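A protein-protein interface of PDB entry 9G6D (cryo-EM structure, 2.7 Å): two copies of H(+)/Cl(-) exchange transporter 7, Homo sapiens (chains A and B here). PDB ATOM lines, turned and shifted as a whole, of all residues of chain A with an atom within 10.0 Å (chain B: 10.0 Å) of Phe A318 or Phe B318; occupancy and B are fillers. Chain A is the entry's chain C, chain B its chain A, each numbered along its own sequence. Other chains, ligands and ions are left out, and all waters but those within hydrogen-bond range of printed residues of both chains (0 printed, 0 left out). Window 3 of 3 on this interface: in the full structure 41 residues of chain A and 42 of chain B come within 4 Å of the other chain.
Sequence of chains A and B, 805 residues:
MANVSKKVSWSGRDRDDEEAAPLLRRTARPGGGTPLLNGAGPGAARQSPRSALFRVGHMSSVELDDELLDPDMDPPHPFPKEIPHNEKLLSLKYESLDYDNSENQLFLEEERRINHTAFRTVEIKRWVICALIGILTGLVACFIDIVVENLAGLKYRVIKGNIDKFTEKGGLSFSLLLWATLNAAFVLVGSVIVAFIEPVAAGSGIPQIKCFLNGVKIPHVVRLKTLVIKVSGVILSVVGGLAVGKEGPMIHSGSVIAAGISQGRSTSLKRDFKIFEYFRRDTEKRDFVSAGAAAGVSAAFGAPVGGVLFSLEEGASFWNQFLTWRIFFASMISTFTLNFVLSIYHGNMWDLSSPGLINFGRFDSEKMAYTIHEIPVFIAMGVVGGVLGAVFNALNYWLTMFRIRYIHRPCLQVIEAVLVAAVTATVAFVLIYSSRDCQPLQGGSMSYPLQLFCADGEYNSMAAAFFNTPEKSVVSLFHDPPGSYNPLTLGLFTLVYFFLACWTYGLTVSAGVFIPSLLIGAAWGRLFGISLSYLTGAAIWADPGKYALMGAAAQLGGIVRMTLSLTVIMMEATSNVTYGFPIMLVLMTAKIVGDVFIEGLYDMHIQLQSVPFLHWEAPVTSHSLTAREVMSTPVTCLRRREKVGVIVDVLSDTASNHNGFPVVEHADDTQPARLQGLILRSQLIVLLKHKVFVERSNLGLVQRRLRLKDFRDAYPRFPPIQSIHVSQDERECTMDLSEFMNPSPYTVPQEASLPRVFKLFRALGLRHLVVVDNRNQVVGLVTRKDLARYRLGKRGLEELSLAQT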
ATOM      1  N   ASP A 287      29.462  41.026  -8.353  1.00  0.00           N
ATOM      2  CA  ASP A 287      30.093  39.791  -7.905  1.00  0.00           C
ATOM      3  C   ASP A 287      31.023  40.040  -6.725  1.00  0.00           C
ATOM      4  O   ASP A 287      31.035  39.267  -5.760  1.00  0.00           O
ATOM      5  CB  ASP A 287      30.857  39.147  -9.061  1.00  0.00           C
ATOM      6  CG  ASP A 287      29.961  38.821 -10.238  1.00  0.00           C
ATOM      7  OD1 ASP A 287      28.725  38.897 -10.082  1.00  0.00           O
ATOM      8  OD2 ASP A 287      30.494  38.489 -11.318  1.00  0.00           O
ATOM      9  N   SER A 311      25.284  34.946   0.348  1.00  0.00           N
ATOM     10  CA  SER A 311      25.497  35.567  -0.952  1.00  0.00           C
ATOM     11  C   SER A 311      24.745  34.836  -2.055  1.00  0.00           C
ATOM     12  O   SER A 311      24.390  35.445  -3.069  1.00  0.00           O
ATOM     13  CB  SER A 311      26.991  35.616  -1.268  1.00  0.00           C
ATOM     14  OG  SER A 311      27.551  36.855  -0.876  1.00  0.00           O
ATOM     15  N   LEU A 312      24.500  33.537  -1.881  1.00  0.00           N
ATOM     16  CA  LEU A 312      23.876  32.749  -2.939  1.00  0.00           C
ATOM     17  C   LEU A 312      22.393  33.080  -3.087  1.00  0.00           C
ATOM     18  O   LEU A 312      21.913  33.328  -4.198  1.00  0.00           O
ATOM     19  CB  LEU A 312      24.075  31.259  -2.659  1.00  0.00           C
ATOM     20  CG  LEU A 312      25.339  30.610  -3.232  1.00  0.00           C
ATOM     21  CD1 LEU A 312      25.136  29.118  -3.425  1.00  0.00           C
ATOM     22  CD2 LEU A 312      25.748  31.262  -4.544  1.00  0.00           C
ATOM     23  N   GLU A 313      21.650  33.090  -1.977  1.00  0.00           N
ATOM     24  CA  GLU A 313      20.211  33.323  -2.065  1.00  0.00           C
ATOM     25  C   GLU A 313      19.902  34.769  -2.430  1.00  0.00           C
ATOM     26  O   GLU A 313      18.986  35.038  -3.216  1.00  0.00           O
ATOM     27  CB  GLU A 313      19.523  32.933  -0.758  1.00  0.00           C
ATOM     28  CG  GLU A 313      20.274  31.904   0.057  1.00  0.00           C
ATOM     29  CD  GLU A 313      19.562  31.552   1.344  1.00  0.00           C
ATOM     30  OE1 GLU A 313      18.317  31.479   1.328  1.00  0.00           O
ATOM     31  OE2 GLU A 313      20.246  31.349   2.369  1.00  0.00           O
ATOM     32  N   GLU A 314      20.650  35.718  -1.864  1.00  0.00           N
ATOM     33  CA  GLU A 314      20.452  37.117  -2.225  1.00  0.00           C
ATOM     34  C   GLU A 314      20.821  37.377  -3.679  1.00  0.00           C
ATOM     35  O   GLU A 314      20.251  38.274  -4.311  1.00  0.00           O
ATOM     36  CB  GLU A 314      21.260  38.020  -1.293  1.00  0.00           C
ATOM     37  CG  GLU A 314      20.563  38.395   0.017  1.00  0.00           C
ATOM     38  CD  GLU A 314      20.012  37.208   0.803  1.00  0.00           C
ATOM     39  OE1 GLU A 314      20.474  36.066   0.604  1.00  0.00           O
ATOM     40  OE2 GLU A 314      19.103  37.422   1.632  1.00  0.00           O
ATOM     41  N   GLY A 315      21.766  36.618  -4.222  1.00  0.00           N
ATOM     42  CA  GLY A 315      22.079  36.707  -5.633  1.00  0.00           C
ATOM     43  C   GLY A 315      20.965  36.138  -6.486  1.00  0.00           C
ATOM     44  O   GLY A 315      20.421  36.832  -7.351  1.00  0.00           O
ATOM     45  N   ALA A 316      20.619  34.874  -6.239  1.00  0.00           N
ATOM     46  CA  ALA A 316      19.532  34.189  -6.937  1.00  0.00           C
ATOM     47  C   ALA A 316      19.720  34.248  -8.451  1.00  0.00           C
ATOM     48  O   ALA A 316      18.797  34.548  -9.210  1.00  0.00           O
ATOM     49  CB  ALA A 316      18.174  34.761  -6.529  1.00  0.00           C
ATOM     50  N   SER A 317      20.937  33.956  -8.890  1.00  0.00           N
ATOM     51  CA  SER A 317      21.297  33.984 -10.300  1.00  0.00           C
ATOM     52  C   SER A 317      21.736  32.589 -10.742  1.00  0.00           C
ATOM     53  O   SER A 317      21.656  31.619  -9.984  1.00  0.00           O
ATOM     54  CB  SER A 317      22.389  35.026 -10.551  1.00  0.00           C
ATOM     55  OG  SER A 317      21.827  36.286 -10.869  1.00  0.00           O
ATOM     56  N   PHE A 318      22.199  32.496 -11.987  1.00  0.00           N
ATOM     57  CA  PHE A 318      22.708  31.235 -12.504  1.00  0.00           C
ATOM     58  C   PHE A 318      23.933  30.791 -11.716  1.00  0.00           C
ATOM     59  O   PHE A 318      24.731  31.610 -11.251  1.00  0.00           O
ATOM     60  CB  PHE A 318      23.062  31.367 -13.986  1.00  0.00           C
ATOM     61  CG  PHE A 318      22.746  30.143 -14.796  1.00  0.00           C
ATOM     62  CD1 PHE A 318      21.437  29.815 -15.102  1.00  0.00           C
ATOM     63  CD2 PHE A 318      23.762  29.319 -15.250  1.00  0.00           C
ATOM     64  CE1 PHE A 318      21.147  28.688 -15.847  1.00  0.00           C
ATOM     65  CE2 PHE A 318      23.478  28.191 -15.995  1.00  0.00           C
ATOM     66  CZ  PHE A 318      22.168  27.876 -16.294  1.00  0.00           C
ATOM     67  N   TRP A 319      24.078  29.478 -11.565  1.00  0.00           N
ATOM     68  CA  TRP A 319      25.193  28.932 -10.806  1.00  0.00           C
ATOM     69  C   TRP A 319      26.502  29.199 -11.537  1.00  0.00           C
ATOM     70  O   TRP A 319      26.678  28.784 -12.688  1.00  0.00           O
ATOM     71  CB  TRP A 319      25.004  27.435 -10.581  1.00  0.00           C
ATOM     72  CG  TRP A 319      26.152  26.812  -9.855  1.00  0.00           C
ATOM     73  CD1 TRP A 319      27.230  26.188 -10.407  1.00  0.00           C
ATOM     74  CD2 TRP A 319      26.345  26.767  -8.438  1.00  0.00           C
ATOM     75  NE1 TRP A 319      28.081  25.752  -9.422  1.00  0.00           N
ATOM     76  CE2 TRP A 319      27.559  26.096  -8.204  1.00  0.00           C
ATOM     77  CE3 TRP A 319      25.608  27.226  -7.344  1.00  0.00           C
ATOM     78  CZ2 TRP A 319      28.052  25.874  -6.922  1.00  0.00           C
ATOM     79  CZ3 TRP A 319      26.098  27.002  -6.073  1.00  0.00           C
ATOM     80  CH2 TRP A 319      27.308  26.332  -5.872  1.00  0.00           C
ATOM     81  N   ASN A 320      27.418  29.892 -10.869  1.00  0.00           N
ATOM     82  CA  ASN A 320      28.757  30.153 -11.385  1.00  0.00           C
ATOM     83  C   ASN A 320      29.748  29.451 -10.467  1.00  0.00           C
ATOM     84  O   ASN A 320      29.876  29.813  -9.293  1.00  0.00           O
ATOM     85  CB  ASN A 320      29.032  31.653 -11.460  1.00  0.00           C
ATOM     86  CG  ASN A 320      30.210  31.987 -12.351  1.00  0.00           C
ATOM     87  OD1 ASN A 320      31.063  31.140 -12.618  1.00  0.00           O
ATOM     88  ND2 ASN A 320      30.264  33.227 -12.816  1.00  0.00           N
ATOM     89  N   GLN A 321      30.438  28.441 -10.999  1.00  0.00           N
ATOM     90  CA  GLN A 321      31.372  27.676 -10.180  1.00  0.00           C
ATOM     91  C   GLN A 321      32.533  28.541  -9.706  1.00  0.00           C
ATOM     92  O   GLN A 321      32.927  28.475  -8.537  1.00  0.00           O
ATOM     93  CB  GLN A 321      31.889  26.470 -10.963  1.00  0.00           C
ATOM     94  CG  GLN A 321      32.817  25.569 -10.169  1.00  0.00           C
ATOM     95  CD  GLN A 321      32.101  24.827  -9.060  1.00  0.00           C
ATOM     96  OE1 GLN A 321      30.966  24.380  -9.228  1.00  0.00           O
ATOM     97  NE2 GLN A 321      32.761  24.692  -7.916  1.00  0.00           N
ATOM     98  N   PHE A 322      33.091  29.360 -10.598  1.00  0.00           N
ATOM     99  CA  PHE A 322      34.234  30.185 -10.223  1.00  0.00           C
ATOM    100  C   PHE A 322      33.827  31.307  -9.278  1.00  0.00           C
ATOM    101  O   PHE A 322      34.546  31.605  -8.317  1.00  0.00           O
ATOM    102  CB  PHE A 322      34.907  30.749 -11.472  1.00  0.00           C
ATOM    103  CG  PHE A 322      35.445  29.696 -12.392  1.00  0.00           C
ATOM    104  CD1 PHE A 322      36.567  28.965 -12.045  1.00  0.00           C
ATOM    105  CD2 PHE A 322      34.828  29.433 -13.603  1.00  0.00           C
ATOM    106  CE1 PHE A 322      37.066  27.994 -12.888  1.00  0.00           C
ATOM    107  CE2 PHE A 322      35.321  28.462 -14.450  1.00  0.00           C
ATOM    108  CZ  PHE A 322      36.442  27.741 -14.092  1.00  0.00           C
ATOM    109  N   LEU A 323      32.684  31.947  -9.536  1.00  0.00           N
ATOM    110  CA  LEU A 323      32.230  33.020  -8.658  1.00  0.00           C
ATOM    111  C   LEU A 323      31.949  32.501  -7.256  1.00  0.00           C
ATOM    112  O   LEU A 323      32.341  33.126  -6.264  1.00  0.00           O
ATOM    113  CB  LEU A 323      30.987  33.688  -9.243  1.00  0.00           C
ATOM    114  CG  LEU A 323      30.123  34.472  -8.256  1.00  0.00           C
ATOM    115  CD1 LEU A 323      30.828  35.747  -7.833  1.00  0.00           C
ATOM    116  CD2 LEU A 323      28.766  34.780  -8.861  1.00  0.00           C
ATOM    117  N   THR A 324      31.276  31.354  -7.152  1.00  0.00           N
ATOM    118  CA  THR A 324      31.044  30.750  -5.845  1.00  0.00           C
ATOM    119  C   THR A 324      32.352  30.310  -5.204  1.00  0.00           C
ATOM    120  O   THR A 324      32.456  30.258  -3.974  1.00  0.00           O
ATOM    121  CB  THR A 324      30.090  29.565  -5.979  1.00  0.00           C
ATOM    122  OG1 THR A 324      28.970  29.945  -6.786  1.00  0.00           O
ATOM    123  CG2 THR A 324      29.588  29.126  -4.615  1.00  0.00           C
ATOM    124  N   ILE A 327      33.968  33.521  -3.830  1.00  0.00           N
ATOM    125  CA  ILE A 327      33.176  33.933  -2.677  1.00  0.00           C
ATOM    126  C   ILE A 327      33.547  33.098  -1.458  1.00  0.00           C
ATOM    127  O   ILE A 327      33.703  33.626  -0.351  1.00  0.00           O
ATOM    128  CB  ILE A 327      31.675  33.836  -2.999  1.00  0.00           C
ATOM    129  CG1 ILE A 327      31.241  35.010  -3.875  1.00  0.00           C
ATOM    130  CG2 ILE A 327      30.853  33.796  -1.726  1.00  0.00           C
ATOM    131  CD1 ILE A 327      29.795  34.945  -4.304  1.00  0.00           C
ATOM    132  N   ASN B 214      23.212  16.089 -14.855  1.00  0.00           N
ATOM    133  CA  ASN B 214      23.609  16.917 -15.989  1.00  0.00           C
ATOM    134  C   ASN B 214      22.459  17.047 -16.980  1.00  0.00           C
ATOM    135  O   ASN B 214      22.168  18.146 -17.465  1.00  0.00           O
ATOM    136  CB  ASN B 214      24.849  16.313 -16.654  1.00  0.00           C
ATOM    137  CG  ASN B 214      25.396  17.158 -17.800  1.00  0.00           C
ATOM    138  OD1 ASN B 214      24.735  18.058 -18.315  1.00  0.00           O
ATOM    139  ND2 ASN B 214      26.625  16.859 -18.204  1.00  0.00           N
ATOM    140  N   ARG B 286      14.472  15.146 -11.757  1.00  0.00           N
ATOM    141  CA  ARG B 286      15.814  15.664 -11.518  1.00  0.00           C
ATOM    142  C   ARG B 286      15.911  16.344 -10.160  1.00  0.00           C
ATOM    143  O   ARG B 286      16.902  16.174  -9.441  1.00  0.00           O
ATOM    144  CB  ARG B 286      16.208  16.635 -12.628  1.00  0.00           C
ATOM    145  CG  ARG B 286      16.624  15.969 -13.926  1.00  0.00           C
ATOM    146  CD  ARG B 286      17.309  16.947 -14.875  1.00  0.00           C
ATOM    147  NE  ARG B 286      18.407  17.672 -14.246  1.00  0.00           N
ATOM    148  CZ  ARG B 286      18.314  18.896 -13.744  1.00  0.00           C
ATOM    149  NH1 ARG B 286      17.181  19.577 -13.791  1.00  0.00           N
ATOM    150  NH2 ARG B 286      19.383  19.450 -13.180  1.00  0.00           N
ATOM    151  N   ASP B 287      14.896  17.128  -9.796  1.00  0.00           N
ATOM    152  CA  ASP B 287      14.899  17.787  -8.494  1.00  0.00           C
ATOM    153  C   ASP B 287      14.858  16.771  -7.361  1.00  0.00           C
ATOM    154  O   ASP B 287      15.570  16.917  -6.361  1.00  0.00           O
ATOM    155  CB  ASP B 287      13.719  18.750  -8.393  1.00  0.00           C
ATOM    156  CG  ASP B 287      13.638  19.697  -9.571  1.00  0.00           C
ATOM    157  OD1 ASP B 287      12.615  20.401  -9.701  1.00  0.00           O
ATOM    158  OD2 ASP B 287      14.601  19.740 -10.367  1.00  0.00           O
ATOM    159  N   SER B 311      24.599  18.834  -4.432  1.00  0.00           N
ATOM    160  CA  SER B 311      23.472  18.868  -5.356  1.00  0.00           C
ATOM    161  C   SER B 311      23.447  20.155  -6.171  1.00  0.00           C
ATOM    162  O   SER B 311      22.962  20.155  -7.307  1.00  0.00           O
ATOM    163  CB  SER B 311      22.161  18.700  -4.591  1.00  0.00           C
ATOM    164  OG  SER B 311      21.777  17.338  -4.537  1.00  0.00           O
ATOM    165  N   LEU B 312      23.951  21.256  -5.611  1.00  0.00           N
ATOM    166  CA  LEU B 312      23.892  22.537  -6.308  1.00  0.00           C
ATOM    167  C   LEU B 312      24.839  22.571  -7.503  1.00  0.00           C
ATOM    168  O   LEU B 312      24.445  22.966  -8.605  1.00  0.00           O
ATOM    169  CB  LEU B 312      24.207  23.673  -5.337  1.00  0.00           C
ATOM    170  CG  LEU B 312      23.095  24.060  -4.360  1.00  0.00           C
ATOM    171  CD1 LEU B 312      23.309  25.470  -3.842  1.00  0.00           C
ATOM    172  CD2 LEU B 312      21.728  23.932  -5.013  1.00  0.00           C
ATOM    173  N   GLU B 313      26.096  22.163  -7.305  1.00  0.00           N
ATOM    174  CA  GLU B 313      27.062  22.229  -8.397  1.00  0.00           C
ATOM    175  C   GLU B 313      26.767  21.189  -9.468  1.00  0.00           C
ATOM    176  O   GLU B 313      26.858  21.482 -10.666  1.00  0.00           O
ATOM    177  CB  GLU B 313      28.483  22.057  -7.865  1.00  0.00           C
ATOM    178  CG  GLU B 313      28.666  22.529  -6.446  1.00  0.00           C
ATOM    179  CD  GLU B 313      29.975  22.078  -5.851  1.00  0.00           C
ATOM    180  OE1 GLU B 313      31.026  22.307  -6.485  1.00  0.00           O
ATOM    181  OE2 GLU B 313      29.957  21.505  -4.746  1.00  0.00           O
ATOM    182  N   GLU B 314      26.421  19.968  -9.060  1.00  0.00           N
ATOM    183  CA  GLU B 314      26.068  18.941 -10.033  1.00  0.00           C
ATOM    184  C   GLU B 314      24.800  19.307 -10.793  1.00  0.00           C
ATOM    185  O   GLU B 314      24.599  18.847 -11.922  1.00  0.00           O
ATOM    186  CB  GLU B 314      25.918  17.592  -9.332  1.00  0.00           C
ATOM    187  CG  GLU B 314      27.227  16.821  -9.106  1.00  0.00           C
ATOM    188  CD  GLU B 314      28.365  17.646  -8.507  1.00  0.00           C
ATOM    189  OE1 GLU B 314      28.111  18.681  -7.855  1.00  0.00           O
ATOM    190  OE2 GLU B 314      29.535  17.249  -8.690  1.00  0.00           O
ATOM    191  N   GLY B 315      23.940  20.127 -10.197  1.00  0.00           N
ATOM    192  CA  GLY B 315      22.793  20.656 -10.906  1.00  0.00           C
ATOM    193  C   GLY B 315      23.187  21.788 -11.830  1.00  0.00           C
ATOM    194  O   GLY B 315      22.904  21.744 -13.032  1.00  0.00           O
ATOM    195  N   ALA B 316      23.850  22.804 -11.272  1.00  0.00           N
ATOM    196  CA  ALA B 316      24.357  23.944 -12.036  1.00  0.00           C
ATOM    197  C   ALA B 316      23.250  24.614 -12.845  1.00  0.00           C
ATOM    198  O   ALA B 316      23.418  24.936 -14.023  1.00  0.00           O
ATOM    199  CB  ALA B 316      25.516  23.524 -12.942  1.00  0.00           C
ATOM    200  N   SER B 317      22.107  24.827 -12.205  1.00  0.00           N
ATOM    201  CA  SER B 317      20.955  25.455 -12.835  1.00  0.00           C
ATOM    202  C   SER B 317      20.622  26.755 -12.103  1.00  0.00           C
ATOM    203  O   SER B 317      21.352  27.195 -11.210  1.00  0.00           O
ATOM    204  CB  SER B 317      19.765  24.494 -12.852  1.00  0.00           C
ATOM    205  OG  SER B 317      19.613  23.847 -11.601  1.00  0.00           O
ATOM    206  N   PHE B 318      19.510  27.371 -12.496  1.00  0.00           N
ATOM    207  CA  PHE B 318      19.068  28.601 -11.856  1.00  0.00           C
ATOM    208  C   PHE B 318      18.742  28.352 -10.389  1.00  0.00           C
ATOM    209  O   PHE B 318      18.252  27.283 -10.017  1.00  0.00           O
ATOM    210  CB  PHE B 318      17.843  29.165 -12.574  1.00  0.00           C
ATOM    211  CG  PHE B 318      17.870  30.657 -12.741  1.00  0.00           C
ATOM    212  CD1 PHE B 318      18.717  31.249 -13.662  1.00  0.00           C
ATOM    213  CD2 PHE B 318      17.052  31.467 -11.973  1.00  0.00           C
ATOM    214  CE1 PHE B 318      18.745  32.623 -13.817  1.00  0.00           C
ATOM    215  CE2 PHE B 318      17.074  32.841 -12.123  1.00  0.00           C
ATOM    216  CZ  PHE B 318      17.923  33.419 -13.046  1.00  0.00           C
ATOM    217  N   TRP B 319      19.027  29.347  -9.554  1.00  0.00           N
ATOM    218  CA  TRP B 319      18.768  29.218  -8.126  1.00  0.00           C
ATOM    219  C   TRP B 319      17.273  29.089  -7.867  1.00  0.00           C
ATOM    220  O   TRP B 319      16.465  29.840  -8.419  1.00  0.00           O
ATOM    221  CB  TRP B 319      19.333  30.422  -7.375  1.00  0.00           C
ATOM    222  CG  TRP B 319      18.998  30.425  -5.916  1.00  0.00           C
ATOM    223  CD1 TRP B 319      17.956  31.066  -5.315  1.00  0.00           C
ATOM    224  CD2 TRP B 319      19.712  29.755  -4.870  1.00  0.00           C
ATOM    225  NE1 TRP B 319      17.975  30.836  -3.962  1.00  0.00           N
ATOM    226  CE2 TRP B 319      19.043  30.034  -3.663  1.00  0.00           C
ATOM    227  CE3 TRP B 319      20.851  28.946  -4.838  1.00  0.00           C
ATOM    228  CZ2 TRP B 319      19.476  29.533  -2.440  1.00  0.00           C
ATOM    229  CZ3 TRP B 319      21.278  28.451  -3.621  1.00  0.00           C
ATOM    230  CH2 TRP B 319      20.592  28.746  -2.439  1.00  0.00           C
ATOM    231  N   ASN B 320      16.911  28.128  -7.022  1.00  0.00           N
ATOM    232  CA  ASN B 320      15.525  27.894  -6.631  1.00  0.00           C
ATOM    233  C   ASN B 320      15.479  27.839  -5.111  1.00  0.00           C
ATOM    234  O   ASN B 320      16.045  26.924  -4.505  1.00  0.00           O
ATOM    235  CB  ASN B 320      14.988  26.604  -7.248  1.00  0.00           C
ATOM    236  CG  ASN B 320      13.476  26.523  -7.208  1.00  0.00           C
ATOM    237  OD1 ASN B 320      12.826  27.190  -6.406  1.00  0.00           O
ATOM    238  ND2 ASN B 320      12.908  25.698  -8.078  1.00  0.00           N
ATOM    239  N   GLN B 321      14.819  28.822  -4.498  1.00  0.00           N
ATOM    240  CA  GLN B 321      14.787  28.897  -3.042  1.00  0.00           C
ATOM    241  C   GLN B 321      14.061  27.700  -2.441  1.00  0.00           C
ATOM    242  O   GLN B 321      14.522  27.114  -1.455  1.00  0.00           O
ATOM    243  CB  GLN B 321      14.128  30.203  -2.598  1.00  0.00           C
ATOM    244  CG  GLN B 321      14.111  30.408  -1.095  1.00  0.00           C
ATOM    245  CD  GLN B 321      15.494  30.649  -0.526  1.00  0.00           C
ATOM    246  OE1 GLN B 321      16.317  31.335  -1.131  1.00  0.00           O
ATOM    247  NE2 GLN B 321      15.757  30.084   0.647  1.00  0.00           N
ATOM    248  N   PHE B 322      12.924  27.321  -3.025  1.00  0.00           N
ATOM    249  CA  PHE B 322      12.144  26.223  -2.463  1.00  0.00           C
ATOM    250  C   PHE B 322      12.800  24.877  -2.737  1.00  0.00           C
ATOM    251  O   PHE B 322      12.780  23.988  -1.878  1.00  0.00           O
ATOM    252  CB  PHE B 322      10.723  26.256  -3.017  1.00  0.00           C
ATOM    253  CG  PHE B 322       9.839  27.267  -2.350  1.00  0.00           C
ATOM    254  CD1 PHE B 322       9.091  28.157  -3.101  1.00  0.00           C
ATOM    255  CD2 PHE B 322       9.761  27.331  -0.969  1.00  0.00           C
ATOM    256  CE1 PHE B 322       8.279  29.090  -2.488  1.00  0.00           C
ATOM    257  CE2 PHE B 322       8.952  28.262  -0.350  1.00  0.00           C
ATOM    258  CZ  PHE B 322       8.209  29.143  -1.111  1.00  0.00           C
ATOM    259  N   LEU B 323      13.379  24.703  -3.925  1.00  0.00           N
ATOM    260  CA  LEU B 323      14.057  23.448  -4.237  1.00  0.00           C
ATOM    261  C   LEU B 323      15.268  23.243  -3.338  1.00  0.00           C
ATOM    262  O   LEU B 323      15.476  22.152  -2.796  1.00  0.00           O
ATOM    263  CB  LEU B 323      14.469  23.422  -5.707  1.00  0.00           C
ATOM    264  CG  LEU B 323      15.397  22.275  -6.103  1.00  0.00           C
ATOM    265  CD1 LEU B 323      14.751  20.937  -5.794  1.00  0.00           C
ATOM    266  CD2 LEU B 323      15.764  22.367  -7.573  1.00  0.00           C
ATOM    267  N   THR B 324      16.081  24.288  -3.163  1.00  0.00           N
ATOM    268  CA  THR B 324      17.217  24.192  -2.255  1.00  0.00           C
ATOM    269  C   THR B 324      16.762  23.953  -0.824  1.00  0.00           C
ATOM    270  O   THR B 324      17.529  23.434  -0.005  1.00  0.00           O
ATOM    271  CB  THR B 324      18.069  25.458  -2.339  1.00  0.00           C
ATOM    272  OG1 THR B 324      18.123  25.909  -3.697  1.00  0.00           O
ATOM    273  CG2 THR B 324      19.481  25.186  -1.848  1.00  0.00           C
ATOM    274  N   ILE B 327      15.945  20.116  -0.791  1.00  0.00           N
ATOM    275  CA  ILE B 327      17.233  19.429  -0.779  1.00  0.00           C
ATOM    276  C   ILE B 327      17.856  19.502   0.607  1.00  0.00           C
ATOM    277  O   ILE B 327      18.375  18.507   1.127  1.00  0.00           O
ATOM    278  CB  ILE B 327      18.160  20.032  -1.850  1.00  0.00           C
ATOM    279  CG1 ILE B 327      17.739  19.570  -3.245  1.00  0.00           C
ATOM    280  CG2 ILE B 327      19.605  19.668  -1.578  1.00  0.00           C
ATOM    281  CD1 ILE B 327      18.412  20.330  -4.362  1.00  0.00           C
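NE2 of Gln B321 sits at hydrogen-bond distance from OE1 of Glu A313 (3.0 Å).
The side-chain amide nitrogen (NE2) of Gln A321 lies within hydrogen-bond range of the side-chain carboxylate (OE1) of Glu B313, 3.3 Å away.
The indole nitrogen (NE1) of Trp A319 lies within hydrogen-bond range of the side-chain amide oxygen (OE1) of Gln A321, at 3.2 Å.
The side-chain amide oxygen (OE1) of Gln B321 lies within hydrogen-bond range of the indole nitrogen (NE1) of Trp B319.
Among the printed residues, pairs that only touch across the chains: Leu A312 with Trp B319 (3.9 Å), Glu A313 with Trp B319 (3.5 Å), Ala A316 with Phe B318 (3.8 Å), Ala A316 with Trp B319 (3.8 Å), Ser A317 with Trp B319 (3.5 Å), Phe A318 with Ala B316 (3.8 Å), Phe A318 with Phe B318 (3.4 Å), Trp A319 with Leu B312 (3.9 Å), Trp A319 with Glu B313 (3.4 Å), Trp A319 with Ala B316 (3.8 Å) and Trp A319 with Ser B317 (3.6 Å).
Phe A318 touches just these residues of chain B: Ala B316 and Phe B318.
Phe B318 touches just these residues of chain A: Ala A316 and Phe A318.
Of chain B, only Trp B319 (3.5 Å) comes within 4 Å of Ser A317.
Of the printed residues of chain B, Leu A312 touches Trp B319.
Of the printed residues of chain A, Trp B319 touches Leu A312, Glu A313, Ala A316 and Ser A317.
Printed residues of chain A within 4 Å of Leu B312: Trp A319.
Of the printed residues of chain B, Ala A316 touches Phe B318 (3.8 Å) and Trp B319 (3.8 Å).
Asn B320 touches none of the printed residues of chain A.
The nearest residue of chain B that does not touch Phe A318 is Ser B317 (4.2 Å).
Of the 18 printed residues of chain B, 7 touch a printed residue of chain A.
Along chain B the printed residues that touch a printed residue of chain A span positions 312 to 321.
Of the 16 printed residues of chain A, 7 touch a printed residue of chain B.
Printed residues of chain A that touch a printed residue of chain B: Leu A312, Glu A313, Ala A316, Ser A317, Phe A318, Trp A319 and Gln A321.
Among the printed residues, 13 pairs touch across the chains.
Among the printed residues, no Asp or Glu carboxylate lies within 4 Å of a Lys or Arg side-chain nitrogen of the other chain.
Glu A313 touches Trp B319, and with the chains exchanged Trp A319 touches Glu B313.
Glu A313 touches Gln B321, and with the chains exchanged Gln A321 touches Glu B313.
Ala A316 touches Phe B318, and with the chains exchanged Phe A318 touches Ala B316.
Phe B318 touches its own counterpart, Phe A318.
Positions printed for both chains: 287, 311, 312, 313, 314, 315, 316, 317, 318, 319, 320, 321, 322, 323, 324 and 327.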
